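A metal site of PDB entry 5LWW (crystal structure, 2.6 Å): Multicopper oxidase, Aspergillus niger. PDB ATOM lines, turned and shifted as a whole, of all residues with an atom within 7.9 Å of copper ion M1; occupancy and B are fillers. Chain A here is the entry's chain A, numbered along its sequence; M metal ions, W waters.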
ATOM      1  N   HIS A  81       6.584   5.962  -4.114  1.00  0.00           N
ATOM      2  CA  HIS A  81       7.097   7.077  -3.326  1.00  0.00           C
ATOM      3  C   HIS A  81       7.976   7.937  -4.248  1.00  0.00           C
ATOM      4  O   HIS A  81       8.711   7.416  -5.108  1.00  0.00           O
ATOM      5  CB  HIS A  81       7.864   6.527  -2.120  1.00  0.00           C
ATOM      6  CG  HIS A  81       8.595   7.578  -1.337  1.00  0.00           C
ATOM      7  ND1 HIS A  81       7.941   8.593  -0.664  1.00  0.00           N
ATOM      8  CD2 HIS A  81       9.912   7.785  -1.130  1.00  0.00           C
ATOM      9  CE1 HIS A  81       8.818   9.373  -0.075  1.00  0.00           C
ATOM     10  NE2 HIS A  81      10.024   8.910  -0.342  1.00  0.00           N
ATOM     11  N   HIS A  83      10.856  10.033  -3.904  1.00  0.00           N
ATOM     12  CA  HIS A  83      11.903  10.290  -2.933  1.00  0.00           C
ATOM     13  C   HIS A  83      12.373  11.781  -2.938  1.00  0.00           C
ATOM     14  O   HIS A  83      12.671  12.374  -3.989  1.00  0.00           O
ATOM     15  CB  HIS A  83      13.048   9.259  -3.158  1.00  0.00           C
ATOM     16  CG  HIS A  83      14.149   9.321  -2.154  1.00  0.00           C
ATOM     17  ND1 HIS A  83      14.491   8.245  -1.342  1.00  0.00           N
ATOM     18  CD2 HIS A  83      15.020  10.308  -1.828  1.00  0.00           C
ATOM     19  CE1 HIS A  83      15.502   8.576  -0.571  1.00  0.00           C
ATOM     20  NE2 HIS A  83      15.835   9.826  -0.830  1.00  0.00           N
ATOM     21  N   GLY A  84      12.415  12.416  -1.760  1.00  0.00           N
ATOM     22  CA  GLY A  84      12.923  13.785  -1.675  1.00  0.00           C
ATOM     23  C   GLY A  84      11.880  14.863  -1.983  1.00  0.00           C
ATOM     24  O   GLY A  84      12.104  16.052  -1.714  1.00  0.00           O
ATOM     25  N   ASP A  94       2.483  10.489  -0.608  1.00  0.00           N
ATOM     26  CA  ASP A  94       3.876  10.190  -0.393  1.00  0.00           C
ATOM     27  C   ASP A  94       4.118   8.699  -0.699  1.00  0.00           C
ATOM     28  O   ASP A  94       5.262   8.287  -0.921  1.00  0.00           O
ATOM     29  CB  ASP A  94       4.244  10.580   1.054  1.00  0.00           C
ATOM     30  CG  ASP A  94       5.714  10.530   1.336  1.00  0.00           C
ATOM     31  OD1 ASP A  94       6.499  11.178   0.642  1.00  0.00           O
ATOM     32  OD2 ASP A  94       6.109   9.850   2.301  1.00  0.00           O
ATOM     33  N   GLY A  95       3.045   7.908  -0.694  1.00  0.00           N
ATOM     34  CA  GLY A  95       3.112   6.503  -1.181  1.00  0.00           C
ATOM     35  C   GLY A  95       3.857   5.476  -0.308  1.00  0.00           C
ATOM     36  O   GLY A  95       4.512   4.567  -0.807  1.00  0.00           O
ATOM     37  N   VAL A  96       3.779   5.628   1.016  1.00  0.00           N
ATOM     38  CA  VAL A  96       4.318   4.616   1.923  1.00  0.00           C
ATOM     39  C   VAL A  96       3.191   3.686   2.397  1.00  0.00           C
ATOM     40  O   VAL A  96       2.394   4.056   3.239  1.00  0.00           O
ATOM     41  CB  VAL A  96       5.000   5.319   3.121  1.00  0.00           C
ATOM     42  CG1 VAL A  96       5.472   4.324   4.150  1.00  0.00           C
ATOM     43  CG2 VAL A  96       6.138   6.186   2.635  1.00  0.00           C
ATOM     44  N   HIS A 125      10.262   5.256  -6.465  1.00  0.00           N
ATOM     45  CA  HIS A 125      10.477   3.821  -6.433  1.00  0.00           C
ATOM     46  C   HIS A 125       9.418   3.251  -5.539  1.00  0.00           C
ATOM     47  O   HIS A 125       8.707   4.017  -4.919  1.00  0.00           O
ATOM     48  CB  HIS A 125      11.878   3.473  -5.903  1.00  0.00           C
ATOM     49  CG  HIS A 125      12.224   4.123  -4.583  1.00  0.00           C
ATOM     50  ND1 HIS A 125      11.622   3.770  -3.391  1.00  0.00           N
ATOM     51  CD2 HIS A 125      13.162   5.052  -4.270  1.00  0.00           C
ATOM     52  CE1 HIS A 125      12.161   4.474  -2.411  1.00  0.00           C
ATOM     53  NE2 HIS A 125      13.093   5.266  -2.920  1.00  0.00           N
ATOM     54  N   SER A 126       9.316   1.936  -5.455  1.00  0.00           N
ATOM     55  CA  SER A 126       8.304   1.354  -4.599  1.00  0.00           C
ATOM     56  C   SER A 126       8.665   1.519  -3.154  1.00  0.00           C
ATOM     57  O   SER A 126       9.839   1.467  -2.767  1.00  0.00           O
ATOM     58  CB  SER A 126       8.057  -0.122  -4.860  1.00  0.00           C
ATOM     59  OG  SER A 126       7.654  -0.302  -6.187  1.00  0.00           O
ATOM     60  N   HIS A 127       7.628   1.730  -2.358  1.00  0.00           N
ATOM     61  CA  HIS A 127       7.808   1.631  -0.958  1.00  0.00           C
ATOM     62  C   HIS A 127       6.894   0.478  -0.571  1.00  0.00           C
ATOM     63  O   HIS A 127       6.020   0.612   0.266  1.00  0.00           O
ATOM     64  CB  HIS A 127       7.436   2.954  -0.311  1.00  0.00           C
ATOM     65  CG  HIS A 127       8.453   3.430   0.676  1.00  0.00           C
ATOM     66  ND1 HIS A 127       8.693   2.775   1.861  1.00  0.00           N
ATOM     67  CD2 HIS A 127       9.309   4.483   0.642  1.00  0.00           C
ATOM     68  CE1 HIS A 127       9.646   3.417   2.528  1.00  0.00           C
ATOM     69  NE2 HIS A 127      10.023   4.470   1.814  1.00  0.00           N
ATOM     70  N   TRP A 133      13.724  -2.654  -5.293  1.00  0.00           N
ATOM     71  CA  TRP A 133      14.935  -3.386  -5.721  1.00  0.00           C
ATOM     72  C   TRP A 133      14.717  -4.548  -6.711  1.00  0.00           C
ATOM     73  O   TRP A 133      15.685  -5.184  -7.131  1.00  0.00           O
ATOM     74  CB  TRP A 133      15.793  -3.761  -4.512  1.00  0.00           C
ATOM     75  CG  TRP A 133      16.077  -2.535  -3.770  1.00  0.00           C
ATOM     76  CD1 TRP A 133      17.113  -1.680  -3.961  1.00  0.00           C
ATOM     77  CD2 TRP A 133      15.255  -1.938  -2.772  1.00  0.00           C
ATOM     78  NE1 TRP A 133      17.001  -0.602  -3.108  1.00  0.00           N
ATOM     79  CE2 TRP A 133      15.868  -0.748  -2.370  1.00  0.00           C
ATOM     80  CE3 TRP A 133      14.052  -2.322  -2.172  1.00  0.00           C
ATOM     81  CZ2 TRP A 133      15.329   0.068  -1.401  1.00  0.00           C
ATOM     82  CZ3 TRP A 133      13.504  -1.487  -1.182  1.00  0.00           C
ATOM     83  CH2 TRP A 133      14.140  -0.310  -0.818  1.00  0.00           C
ATOM     84  N   HIS A 424      17.089   8.282   5.885  1.00  0.00           N
ATOM     85  CA  HIS A 424      16.333   9.082   4.979  1.00  0.00           C
ATOM     86  C   HIS A 424      15.092   9.547   5.688  1.00  0.00           C
ATOM     87  O   HIS A 424      14.422   8.752   6.337  1.00  0.00           O
ATOM     88  CB  HIS A 424      15.961   8.226   3.782  1.00  0.00           C
ATOM     89  CG  HIS A 424      14.974   8.874   2.880  1.00  0.00           C
ATOM     90  ND1 HIS A 424      15.044  10.208   2.551  1.00  0.00           N
ATOM     91  CD2 HIS A 424      13.908   8.378   2.212  1.00  0.00           C
ATOM     92  CE1 HIS A 424      14.060  10.507   1.727  1.00  0.00           C
ATOM     93  NE2 HIS A 424      13.370   9.410   1.498  1.00  0.00           N
ATOM     94  N   LEU A 425      14.793  10.829   5.613  1.00  0.00           N
ATOM     95  CA  LEU A 425      13.587  11.352   6.251  1.00  0.00           C
ATOM     96  C   LEU A 425      12.623  11.781   5.147  1.00  0.00           C
ATOM     97  O   LEU A 425      13.007  12.565   4.272  1.00  0.00           O
ATOM     98  CB  LEU A 425      13.880  12.526   7.210  1.00  0.00           C
ATOM     99  CG  LEU A 425      12.719  13.344   7.818  1.00  0.00           C
ATOM    100  CD1 LEU A 425      11.771  12.517   8.703  1.00  0.00           C
ATOM    101  CD2 LEU A 425      13.209  14.569   8.589  1.00  0.00           C
ATOM    102  N   HIS A 426      11.406  11.211   5.181  1.00  0.00           N
ATOM    103  CA  HIS A 426      10.322  11.582   4.291  1.00  0.00           C
ATOM    104  C   HIS A 426       9.810  12.952   4.719  1.00  0.00           C
ATOM    105  O   HIS A 426       9.945  13.330   5.876  1.00  0.00           O
ATOM    106  CB  HIS A 426       9.179  10.574   4.395  1.00  0.00           C
ATOM    107  CG  HIS A 426       9.442   9.264   3.710  1.00  0.00           C
ATOM    108  ND1 HIS A 426       8.583   8.733   2.773  1.00  0.00           N
ATOM    109  CD2 HIS A 426      10.472   8.382   3.826  1.00  0.00           C
ATOM    110  CE1 HIS A 426       9.071   7.572   2.340  1.00  0.00           C
ATOM    111  NE2 HIS A 426      10.216   7.351   2.953  1.00  0.00           N
ATOM    112  N   LEU A 486       7.638   8.427   7.291  1.00  0.00           N
ATOM    113  CA  LEU A 486       8.585   7.358   7.558  1.00  0.00           C
ATOM    114  C   LEU A 486       9.963   7.956   7.730  1.00  0.00           C
ATOM    115  O   LEU A 486      10.352   8.824   6.943  1.00  0.00           O
ATOM    116  CB  LEU A 486       8.601   6.343   6.421  1.00  0.00           C
ATOM    117  CG  LEU A 486       9.063   4.918   6.793  1.00  0.00           C
ATOM    118  CD1 LEU A 486       8.105   4.142   7.704  1.00  0.00           C
ATOM    119  CD2 LEU A 486       9.387   4.121   5.553  1.00  0.00           C
ATOM    120  N   ILE A 487      10.687   7.545   8.780  1.00  0.00           N
ATOM    121  CA  ILE A 487      12.146   7.780   8.860  1.00  0.00           C
ATOM    122  C   ILE A 487      12.841   6.420   8.984  1.00  0.00           C
ATOM    123  O   ILE A 487      12.472   5.598   9.829  1.00  0.00           O
ATOM    124  CB  ILE A 487      12.587   8.775   9.955  1.00  0.00           C
ATOM    125  CG1 ILE A 487      14.109   8.977   9.864  1.00  0.00           C
ATOM    126  CG2 ILE A 487      12.188   8.270  11.322  1.00  0.00           C
ATOM    127  CD1 ILE A 487      14.679  10.161  10.613  1.00  0.00           C
ATOM    128  N   HIS A 488      13.847   6.183   8.151  1.00  0.00           N
ATOM    129  CA  HIS A 488      14.279   4.820   8.005  1.00  0.00           C
ATOM    130  C   HIS A 488      15.607   4.652   7.328  1.00  0.00           C
ATOM    131  O   HIS A 488      16.138   5.571   6.705  1.00  0.00           O
ATOM    132  CB  HIS A 488      13.212   3.999   7.236  1.00  0.00           C
ATOM    133  CG  HIS A 488      13.171   4.271   5.764  1.00  0.00           C
ATOM    134  ND1 HIS A 488      13.676   3.406   4.830  1.00  0.00           N
ATOM    135  CD2 HIS A 488      12.710   5.340   5.067  1.00  0.00           C
ATOM    136  CE1 HIS A 488      13.524   3.913   3.613  1.00  0.00           C
ATOM    137  NE2 HIS A 488      12.942   5.093   3.726  1.00  0.00           N
ATOM    138  N   CYS A 489      16.151   3.454   7.463  1.00  0.00           N
ATOM    139  CA  CYS A 489      17.349   3.101   6.746  1.00  0.00           C
ATOM    140  C   CYS A 489      16.987   2.836   5.302  1.00  0.00           C
ATOM    141  O   CYS A 489      16.035   2.079   5.022  1.00  0.00           O
ATOM    142  CB  CYS A 489      17.966   1.858   7.357  1.00  0.00           C
ATOM    143  SG  CYS A 489      19.386   1.399   6.380  1.00  0.00           S
ATOM    144  N   HIS A 490      17.719   3.472   4.390  1.00  0.00           N
ATOM    145  CA  HIS A 490      17.413   3.335   2.983  1.00  0.00           C
ATOM    146  C   HIS A 490      17.900   2.023   2.387  1.00  0.00           C
ATOM    147  O   HIS A 490      17.704   1.769   1.194  1.00  0.00           O
ATOM    148  CB  HIS A 490      17.888   4.528   2.155  1.00  0.00           C
ATOM    149  CG  HIS A 490      17.037   4.762   0.931  1.00  0.00           C
ATOM    150  ND1 HIS A 490      17.151   4.003  -0.214  1.00  0.00           N
ATOM    151  CD2 HIS A 490      16.039   5.643   0.705  1.00  0.00           C
ATOM    152  CE1 HIS A 490      16.258   4.409  -1.099  1.00  0.00           C
ATOM    153  NE2 HIS A 490      15.568   5.412  -0.562  1.00  0.00           N
ATOM    154  N   ALA A 495      14.988  -2.013   6.147  1.00  0.00           N
ATOM    155  CA  ALA A 495      13.687  -1.354   6.374  1.00  0.00           C
ATOM    156  C   ALA A 495      12.563  -2.376   6.429  1.00  0.00           C
ATOM    157  O   ALA A 495      11.592  -2.204   7.153  1.00  0.00           O
ATOM    158  CB  ALA A 495      13.430  -0.326   5.298  1.00  0.00           C
ATOM    159  N   ILE A 550       6.361  -1.522   5.562  1.00  0.00           N
ATOM    160  CA  ILE A 550       6.769  -0.408   4.647  1.00  0.00           C
ATOM    161  C   ILE A 550       7.589  -0.883   3.414  1.00  0.00           C
ATOM    162  O   ILE A 550       7.640  -2.098   3.142  1.00  0.00           O
ATOM    163  CB  ILE A 550       7.475   0.773   5.377  1.00  0.00           C
ATOM    164  CG1 ILE A 550       8.754   0.310   6.091  1.00  0.00           C
ATOM    165  CG2 ILE A 550       6.526   1.442   6.353  1.00  0.00           C
ATOM    166  CD1 ILE A 550       9.956   0.283   5.189  1.00  0.00           C
ATOM    167  OXT ILE A 550       8.190  -0.069   2.667  1.00  0.00           O
HETATM  168 CU    CU M   1      11.486   5.737   2.207  1.00  0.00          CU
HETATM  169 CU    CU M   2      11.666   9.168   0.572  1.00  0.00          CU
HETATM  170 CU    CU M   3      13.921   6.394  -1.403  1.00  0.00          CU
HETATM  171  O   HOH W   1      12.691   5.967   0.567  1.00  0.00           O
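A ring nitrogen (ND1) of His 127 sits at hydrogen-bond distance from the chain-end carboxylate (OXT) of Ile 550, at 3.0 Å. A ring nitrogen (ND1) of His 426 sits close to a ring nitrogen (ND1) of His 81 (3.5 Å). The backbone NH (N) of His 426 sits at hydrogen-bond distance from the backbone carbonyl oxygen (O) of Leu 486. ND1 of His 426 sits at hydrogen-bond distance from OD2 of Asp 94 (2.8 Å). The backbone NH (N) of His 424 sits at hydrogen-bond distance from the backbone carbonyl oxygen (O) of His 488 (3.0 Å). NE2 of His 83 lies close to ND1 of His 424, 3.5 Å away.
Merely in contact with copper ion M1: His 424 (3.6 Å). The nearest printed residue that does not touch copper ion M1 is His 81 (4.2 Å).
Copper ion M1 is bound by a ring nitrogen (NE2) of His 127 (2.0 Å), water W1 (2.0 Å), a ring nitrogen (NE2) of His 426 (2.2 Å) and a ring nitrogen (NE2) of His 488 (2.2 Å). Copper ion M1 has four donor atoms within binding distance.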
